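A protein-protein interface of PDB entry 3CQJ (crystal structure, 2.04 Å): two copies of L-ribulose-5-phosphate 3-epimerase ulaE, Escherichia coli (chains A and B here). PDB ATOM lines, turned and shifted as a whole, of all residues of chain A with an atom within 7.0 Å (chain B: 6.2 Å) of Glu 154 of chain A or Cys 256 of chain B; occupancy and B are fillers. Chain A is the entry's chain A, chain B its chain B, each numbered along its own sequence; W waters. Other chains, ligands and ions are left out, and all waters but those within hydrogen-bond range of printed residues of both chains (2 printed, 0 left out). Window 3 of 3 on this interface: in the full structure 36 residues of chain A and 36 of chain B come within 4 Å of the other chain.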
ATOM      1  N   ILE A 114      -8.725  13.906 -10.890  1.00  0.00           N
ATOM      2  CA  ILE A 114      -7.968  13.822  -9.642  1.00  0.00           C
ATOM      3  C   ILE A 114      -8.641  14.648  -8.526  1.00  0.00           C
ATOM      4  O   ILE A 114      -8.839  14.142  -7.418  1.00  0.00           O
ATOM      5  CB  ILE A 114      -6.471  14.191  -9.857  1.00  0.00           C
ATOM      6  CG1 ILE A 114      -5.737  13.031 -10.560  1.00  0.00           C
ATOM      7  CG2 ILE A 114      -5.796  14.522  -8.536  1.00  0.00           C
ATOM      8  CD1 ILE A 114      -4.380  13.389 -11.161  1.00  0.00           C
ATOM      9  N   ASP A 147       5.075  11.584 -21.740  1.00  0.00           N
ATOM     10  CA  ASP A 147       5.192  12.853 -21.018  1.00  0.00           C
ATOM     11  C   ASP A 147       3.889  13.264 -20.323  1.00  0.00           C
ATOM     12  O   ASP A 147       3.919  13.826 -19.230  1.00  0.00           O
ATOM     13  CB  ASP A 147       5.688  13.965 -21.955  1.00  0.00           C
ATOM     14  CG  ASP A 147       7.147  13.757 -22.398  1.00  0.00           C
ATOM     15  OD1 ASP A 147       7.859  12.886 -21.820  1.00  0.00           O
ATOM     16  OD2 ASP A 147       7.583  14.469 -23.335  1.00  0.00           O
ATOM     17  N   GLY A 148       2.758  12.982 -20.971  1.00  0.00           N
ATOM     18  CA  GLY A 148       1.439  13.227 -20.392  1.00  0.00           C
ATOM     19  C   GLY A 148       1.204  12.378 -19.153  1.00  0.00           C
ATOM     20  O   GLY A 148       0.620  12.838 -18.161  1.00  0.00           O
ATOM     21  N   LEU A 149       1.654  11.131 -19.226  1.00  0.00           N
ATOM     22  CA  LEU A 149       1.546  10.183 -18.123  1.00  0.00           C
ATOM     23  C   LEU A 149       2.399  10.612 -16.926  1.00  0.00           C
ATOM     24  O   LEU A 149       1.957  10.521 -15.776  1.00  0.00           O
ATOM     25  CB  LEU A 149       1.943   8.790 -18.608  1.00  0.00           C
ATOM     26  CG  LEU A 149       1.550   7.548 -17.816  1.00  0.00           C
ATOM     27  CD1 LEU A 149       0.034   7.499 -17.545  1.00  0.00           C
ATOM     28  CD2 LEU A 149       1.997   6.325 -18.594  1.00  0.00           C
ATOM     29  N   LYS A 150       3.610  11.096 -17.204  1.00  0.00           N
ATOM     30  CA  LYS A 150       4.502  11.583 -16.157  1.00  0.00           C
ATOM     31  C   LYS A 150       3.898  12.806 -15.473  1.00  0.00           C
ATOM     32  O   LYS A 150       3.885  12.887 -14.246  1.00  0.00           O
ATOM     33  CB  LYS A 150       5.905  11.883 -16.708  1.00  0.00           C
ATOM     34  CG  LYS A 150       6.929  12.195 -15.624  1.00  0.00           C
ATOM     35  CD  LYS A 150       8.311  11.673 -15.975  1.00  0.00           C
ATOM     36  CE  LYS A 150       9.234  11.669 -14.752  1.00  0.00           C
ATOM     37  NZ  LYS A 150      10.228  10.544 -14.789  1.00  0.00           N
ATOM     38  N   GLU A 151       3.362  13.727 -16.275  1.00  0.00           N
ATOM     39  CA  GLU A 151       2.654  14.897 -15.766  1.00  0.00           C
ATOM     40  C   GLU A 151       1.448  14.509 -14.901  1.00  0.00           C
ATOM     41  O   GLU A 151       1.251  15.078 -13.827  1.00  0.00           O
ATOM     42  CB  GLU A 151       2.208  15.797 -16.922  1.00  0.00           C
ATOM     43  CG  GLU A 151       1.936  17.236 -16.510  1.00  0.00           C
ATOM     44  CD  GLU A 151       1.654  18.153 -17.699  1.00  0.00           C
ATOM     45  OE1 GLU A 151       2.240  17.941 -18.788  1.00  0.00           O
ATOM     46  OE2 GLU A 151       0.854  19.092 -17.540  1.00  0.00           O
ATOM     47  N   SER A 152       0.666  13.537 -15.368  1.00  0.00           N
ATOM     48  CA  SER A 152      -0.493  13.010 -14.624  1.00  0.00           C
ATOM     49  C   SER A 152      -0.115  12.421 -13.257  1.00  0.00           C
ATOM     50  O   SER A 152      -0.831  12.626 -12.266  1.00  0.00           O
ATOM     51  CB  SER A 152      -1.210  11.934 -15.445  1.00  0.00           C
ATOM     52  OG  SER A 152      -1.623  12.436 -16.710  1.00  0.00           O
ATOM     53  N   VAL A 153       0.995  11.685 -13.221  1.00  0.00           N
ATOM     54  CA  VAL A 153       1.472  11.011 -12.003  1.00  0.00           C
ATOM     55  C   VAL A 153       2.015  12.026 -10.994  1.00  0.00           C
ATOM     56  O   VAL A 153       1.951  11.807  -9.780  1.00  0.00           O
ATOM     57  CB  VAL A 153       2.538   9.924 -12.312  1.00  0.00           C
ATOM     58  CG1 VAL A 153       3.148   9.383 -11.032  1.00  0.00           C
ATOM     59  CG2 VAL A 153       1.925   8.775 -13.079  1.00  0.00           C
ATOM     60  N   GLU A 154       2.551  13.130 -11.511  1.00  0.00           N
ATOM     61  CA  GLU A 154       2.968  14.245 -10.683  1.00  0.00           C
ATOM     62  C   GLU A 154       1.766  14.880  -9.992  1.00  0.00           C
ATOM     63  O   GLU A 154       1.819  15.144  -8.790  1.00  0.00           O
ATOM     64  CB  GLU A 154       3.763  15.269 -11.508  1.00  0.00           C
ATOM     65  CG  GLU A 154       5.175  14.763 -11.842  1.00  0.00           C
ATOM     66  CD  GLU A 154       6.027  15.779 -12.593  1.00  0.00           C
ATOM     67  OE1 GLU A 154       5.714  16.995 -12.541  1.00  0.00           O
ATOM     68  OE2 GLU A 154       7.022  15.357 -13.233  1.00  0.00           O
ATOM     69  N   MET A 155       0.682  15.111 -10.742  1.00  0.00           N
ATOM     70  CA  MET A 155      -0.551  15.615 -10.142  1.00  0.00           C
ATOM     71  C   MET A 155      -1.059  14.621  -9.102  1.00  0.00           C
ATOM     72  O   MET A 155      -1.488  15.021  -8.014  1.00  0.00           O
ATOM     73  CB  MET A 155      -1.661  15.849 -11.173  1.00  0.00           C
ATOM     74  CG  MET A 155      -1.224  16.172 -12.588  1.00  0.00           C
ATOM     75  SD  MET A 155      -2.625  16.588 -13.665  1.00  0.00           S
ATOM     76  CE  MET A 155      -2.880  18.227 -13.022  1.00  0.00           C
ATOM     77  N   ALA A 156      -0.999  13.330  -9.447  1.00  0.00           N
ATOM     78  CA  ALA A 156      -1.419  12.265  -8.545  1.00  0.00           C
ATOM     79  C   ALA A 156      -0.588  12.227  -7.253  1.00  0.00           C
ATOM     80  O   ALA A 156      -1.137  11.986  -6.186  1.00  0.00           O
ATOM     81  CB  ALA A 156      -1.375  10.909  -9.248  1.00  0.00           C
ATOM     82  N   SER A 157       0.724  12.451  -7.361  1.00  0.00           N
ATOM     83  CA  SER A 157       1.623  12.461  -6.189  1.00  0.00           C
ATOM     84  C   SER A 157       1.327  13.610  -5.227  1.00  0.00           C
ATOM     85  O   SER A 157       1.479  13.475  -4.014  1.00  0.00           O
ATOM     86  CB  SER A 157       3.084  12.554  -6.626  1.00  0.00           C
ATOM     87  OG  SER A 157       3.428  11.491  -7.496  1.00  0.00           O
ATOM     88  N   ARG A 158       0.940  14.754  -5.781  1.00  0.00           N
ATOM     89  CA  ARG A 158       0.571  15.909  -4.983  1.00  0.00           C
ATOM     90  C   ARG A 158      -0.738  15.655  -4.242  1.00  0.00           C
ATOM     91  O   ARG A 158      -0.882  16.019  -3.069  1.00  0.00           O
ATOM     92  CB  ARG A 158       0.460  17.153  -5.871  1.00  0.00           C
ATOM     93  CG  ARG A 158       1.795  17.597  -6.441  1.00  0.00           C
ATOM     94  CD  ARG A 158       1.728  18.981  -7.034  1.00  0.00           C
ATOM     95  NE  ARG A 158       1.190  19.004  -8.391  1.00  0.00           N
ATOM     96  CZ  ARG A 158       1.931  19.013  -9.499  1.00  0.00           C
ATOM     97  NH1 ARG A 158       3.257  18.998  -9.430  1.00  0.00           N
ATOM     98  NH2 ARG A 158       1.341  19.041 -10.686  1.00  0.00           N
ATOM     99  N   ALA A 159      -1.666  14.992  -4.928  1.00  0.00           N
ATOM    100  CA  ALA A 159      -3.016  14.774  -4.412  1.00  0.00           C
ATOM    101  C   ALA A 159      -3.086  13.519  -3.554  1.00  0.00           C
ATOM    102  O   ALA A 159      -4.027  13.357  -2.771  1.00  0.00           O
ATOM    103  CB  ALA A 159      -4.004  14.668  -5.562  1.00  0.00           C
ATOM    104  N   GLN A 160      -2.087  12.649  -3.719  1.00  0.00           N
ATOM    105  CA  GLN A 160      -2.055  11.304  -3.119  1.00  0.00           C
ATOM    106  C   GLN A 160      -3.235  10.427  -3.547  1.00  0.00           C
ATOM    107  O   GLN A 160      -3.957   9.864  -2.725  1.00  0.00           O
ATOM    108  CB  GLN A 160      -1.914  11.390  -1.600  1.00  0.00           C
ATOM    109  CG  GLN A 160      -0.612  12.031  -1.170  1.00  0.00           C
ATOM    110  CD  GLN A 160      -0.578  12.342   0.307  1.00  0.00           C
ATOM    111  OE1 GLN A 160      -1.492  12.965   0.837  1.00  0.00           O
ATOM    112  NE2 GLN A 160       0.485  11.908   0.983  1.00  0.00           N
ATOM    113  N   LEU A 163      -3.223   6.251  -9.477  1.00  0.00           N
ATOM    114  CA  LEU A 163      -3.558   6.031 -10.874  1.00  0.00           C
ATOM    115  C   LEU A 163      -3.098   4.624 -11.216  1.00  0.00           C
ATOM    116  O   LEU A 163      -1.993   4.211 -10.849  1.00  0.00           O
ATOM    117  CB  LEU A 163      -2.901   7.063 -11.800  1.00  0.00           C
ATOM    118  CG  LEU A 163      -3.014   8.560 -11.476  1.00  0.00           C
ATOM    119  CD1 LEU A 163      -2.250   9.372 -12.519  1.00  0.00           C
ATOM    120  CD2 LEU A 163      -4.472   9.019 -11.373  1.00  0.00           C
ATOM    121  N   ASN A 188       7.101   5.599  -9.275  1.00  0.00           N
ATOM    122  CA  ASN A 188       6.261   6.424  -8.404  1.00  0.00           C
ATOM    123  C   ASN A 188       5.217   5.549  -7.702  1.00  0.00           C
ATOM    124  O   ASN A 188       4.553   4.729  -8.351  1.00  0.00           O
ATOM    125  CB  ASN A 188       5.594   7.542  -9.219  1.00  0.00           C
ATOM    126  CG  ASN A 188       4.861   8.556  -8.340  1.00  0.00           C
ATOM    127  OD1 ASN A 188       3.828   8.242  -7.738  1.00  0.00           O
ATOM    128  ND2 ASN A 188       5.393   9.776  -8.265  1.00  0.00           N
ATOM    129  N   GLN B  16       4.000  22.766  -8.071  1.00  0.00           N
ATOM    130  CA  GLN B  16       3.555  22.806  -6.647  1.00  0.00           C
ATOM    131  C   GLN B  16       4.480  22.039  -5.718  1.00  0.00           C
ATOM    132  O   GLN B  16       5.090  21.040  -6.100  1.00  0.00           O
ATOM    133  CB  GLN B  16       2.142  22.239  -6.498  1.00  0.00           C
ATOM    134  CG  GLN B  16       1.031  23.278  -6.467  1.00  0.00           C
ATOM    135  CD  GLN B  16      -0.340  22.663  -6.722  1.00  0.00           C
ATOM    136  OE1 GLN B  16      -0.675  21.599  -6.181  1.00  0.00           O
ATOM    137  NE2 GLN B  16      -1.140  23.329  -7.553  1.00  0.00           N
ATOM    138  N   PRO B  18       3.087  20.813  -2.308  1.00  0.00           N
ATOM    139  CA  PRO B  18       1.955  20.812  -1.369  1.00  0.00           C
ATOM    140  C   PRO B  18       2.490  20.866   0.052  1.00  0.00           C
ATOM    141  O   PRO B  18       3.366  20.079   0.405  1.00  0.00           O
ATOM    142  CB  PRO B  18       1.268  19.461  -1.638  1.00  0.00           C
ATOM    143  CG  PRO B  18       1.747  19.047  -2.973  1.00  0.00           C
ATOM    144  CD  PRO B  18       3.145  19.561  -3.082  1.00  0.00           C
ATOM    145  N   ILE B 215      13.024   6.448  -2.826  1.00  0.00           N
ATOM    146  CA  ILE B 215      12.251   7.377  -3.670  1.00  0.00           C
ATOM    147  C   ILE B 215      10.981   6.789  -4.325  1.00  0.00           C
ATOM    148  O   ILE B 215       9.890   7.397  -4.240  1.00  0.00           O
ATOM    149  CB  ILE B 215      13.193   8.188  -4.646  1.00  0.00           C
ATOM    150  CG1 ILE B 215      13.073   9.705  -4.408  1.00  0.00           C
ATOM    151  CG2 ILE B 215      13.090   7.733  -6.101  1.00  0.00           C
ATOM    152  CD1 ILE B 215      11.738  10.333  -4.764  1.00  0.00           C
ATOM    153  N   LEU B 250      15.723  15.176  -2.400  1.00  0.00           N
ATOM    154  CA  LEU B 250      14.357  14.779  -2.758  1.00  0.00           C
ATOM    155  C   LEU B 250      13.954  15.405  -4.091  1.00  0.00           C
ATOM    156  O   LEU B 250      13.368  14.740  -4.941  1.00  0.00           O
ATOM    157  CB  LEU B 250      13.370  15.149  -1.645  1.00  0.00           C
ATOM    158  CG  LEU B 250      13.432  14.332  -0.339  1.00  0.00           C
ATOM    159  CD1 LEU B 250      12.755  15.079   0.797  1.00  0.00           C
ATOM    160  CD2 LEU B 250      12.830  12.930  -0.493  1.00  0.00           C
ATOM    161  N   GLY B 254      13.446  13.395  -7.850  1.00  0.00           N
ATOM    162  CA  GLY B 254      12.143  13.444  -8.512  1.00  0.00           C
ATOM    163  C   GLY B 254      10.950  13.305  -7.585  1.00  0.00           C
ATOM    164  O   GLY B 254       9.869  12.896  -8.019  1.00  0.00           O
ATOM    165  N   TYR B 255      11.132  13.635  -6.307  1.00  0.00           N
ATOM    166  CA  TYR B 255      10.008  13.616  -5.375  1.00  0.00           C
ATOM    167  C   TYR B 255       9.044  14.750  -5.697  1.00  0.00           C
ATOM    168  O   TYR B 255       9.451  15.916  -5.766  1.00  0.00           O
ATOM    169  CB  TYR B 255      10.473  13.713  -3.912  1.00  0.00           C
ATOM    170  CG  TYR B 255       9.310  13.689  -2.947  1.00  0.00           C
ATOM    171  CD1 TYR B 255       8.474  12.569  -2.865  1.00  0.00           C
ATOM    172  CD2 TYR B 255       9.025  14.789  -2.135  1.00  0.00           C
ATOM    173  CE1 TYR B 255       7.395  12.539  -2.001  1.00  0.00           C
ATOM    174  CE2 TYR B 255       7.936  14.768  -1.254  1.00  0.00           C
ATOM    175  CZ  TYR B 255       7.125  13.635  -1.201  1.00  0.00           C
ATOM    176  OH  TYR B 255       6.054  13.600  -0.339  1.00  0.00           O
ATOM    177  N   CYS B 256       7.771  14.404  -5.878  1.00  0.00           N
ATOM    178  CA  CYS B 256       6.738  15.383  -6.215  1.00  0.00           C
ATOM    179  C   CYS B 256       5.583  15.438  -5.235  1.00  0.00           C
ATOM    180  O   CYS B 256       4.514  15.957  -5.569  1.00  0.00           O
ATOM    181  CB  CYS B 256       6.153  15.068  -7.591  1.00  0.00           C
ATOM    182  SG  CYS B 256       7.367  15.098  -8.866  1.00  0.00           S
ATOM    183  N   GLY B 257       5.780  14.900  -4.038  1.00  0.00           N
ATOM    184  CA  GLY B 257       4.679  14.740  -3.100  1.00  0.00           C
ATOM    185  C   GLY B 257       4.600  15.866  -2.099  1.00  0.00           C
ATOM    186  O   GLY B 257       5.353  16.829  -2.185  1.00  0.00           O
ATOM    187  N   PRO B 258       3.685  15.745  -1.130  1.00  0.00           N
ATOM    188  CA  PRO B 258       3.496  16.739  -0.078  1.00  0.00           C
ATOM    189  C   PRO B 258       4.558  16.720   1.021  1.00  0.00           C
ATOM    190  O   PRO B 258       5.233  15.699   1.241  1.00  0.00           O
ATOM    191  CB  PRO B 258       2.124  16.368   0.501  1.00  0.00           C
ATOM    192  CG  PRO B 258       2.016  14.905   0.283  1.00  0.00           C
ATOM    193  CD  PRO B 258       2.740  14.614  -1.004  1.00  0.00           C
HETATM  194  O   HOH W   1       6.817  11.806  -5.921  1.00  0.00           O
HETATM  195  O   HOH W   2      -1.351  20.001  -8.256  1.00  0.00           O
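Among the printed residues, pairs that only touch across the chains: Arg 158 of chain A with Cys 256 of chain B (3.3 Å), Arg 158 of chain A with Gln 16 of chain B (3.3 Å), Gln 160 of chain A with Pro 258 of chain B (3.4 Å), Ser 157 of chain A with Pro 258 of chain B (3.5 Å), Ser 157 of chain A with Gly 257 of chain B (3.6 Å), Arg 158 of chain A with Pro 18 of chain B (3.7 Å), Glu 154 of chain A with Cys 256 of chain B (3.7 Å) and Ser 157 of chain A with Cys 256 of chain B (3.8 Å).
Printed residues of chain B that touch a printed residue of chain A: Gln 16, Pro 18, Cys 256, Gly 257 and Pro 258. Hydrophobic or aromatic side chains of chain B that line the printed part of chain A: Pro 18 and Pro 258. Of the 17 printed residues of chain A, 4 touch a printed residue of chain B. Printed residues of chain A that touch a printed residue of chain B: Glu 154, Ser 157, Arg 158 and Gln 160. Among the printed residues, no Asp or Glu carboxylate lies within 4 Å of a Lys or Arg side-chain nitrogen of the other chain.
Glu 154 of chain A touches just one residue of chain B: Cys 256 (3.7 Å). Cys 256 of chain B touches three residues of chain A. Of the printed residues of chain A, Pro 258 of chain B touches Ser 157 and Gln 160. Printed residues of chain B within 4 Å of Gln 160 of chain A: Pro 258 (3.4 Å). Of the printed residues of chain A, Pro 18 of chain B touches Arg 158 (3.7 Å). Of the printed residues of chain A, Gln 16 of chain B touches Arg 158 (3.3 Å). Of the printed residues of chain B, Ser 157 of chain A touches Cys 256, Gly 257 and Pro 258. Gly 148 of chain A touches none of the printed residues of chain B.
No position is printed for both chains. Of the 8 pairs that touch across the chains among the printed residues, none has its exchanged pair printed and touching as well.
Water W2 bridges the side-chain amide oxygen (OE1) of Gln 16 of chain B (2.7 Å) and the guanidinium group (NE) of Arg 158 of chain A (2.7 Å). Water W1 lies within hydrogen-bond range of the backbone NH of Cys 256 of chain B (2.8 Å) and the side-chain amide nitrogen of Asn 188 of chain A (3.4 Å).
O of Gly 254 of chain B sits at hydrogen-bond distance from SG of Cys 256 of chain B (3.4 Å). The side-chain amide nitrogen (ND2) of Asn 188 of chain A sits at hydrogen-bond distance from the side-chain hydroxyl (OG) of Ser 157 of chain A, 2.7 Å away. The backbone carbonyl oxygen (O) of Val 153 of chain A lies within hydrogen-bond range of the side-chain hydroxyl (OG) of Ser 157 of chain A. The side-chain hydroxyl (OH) of Tyr 255 of chain B lies within hydrogen-bond range of the backbone carbonyl oxygen (O) of Pro 258 of chain B (2.8 Å).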
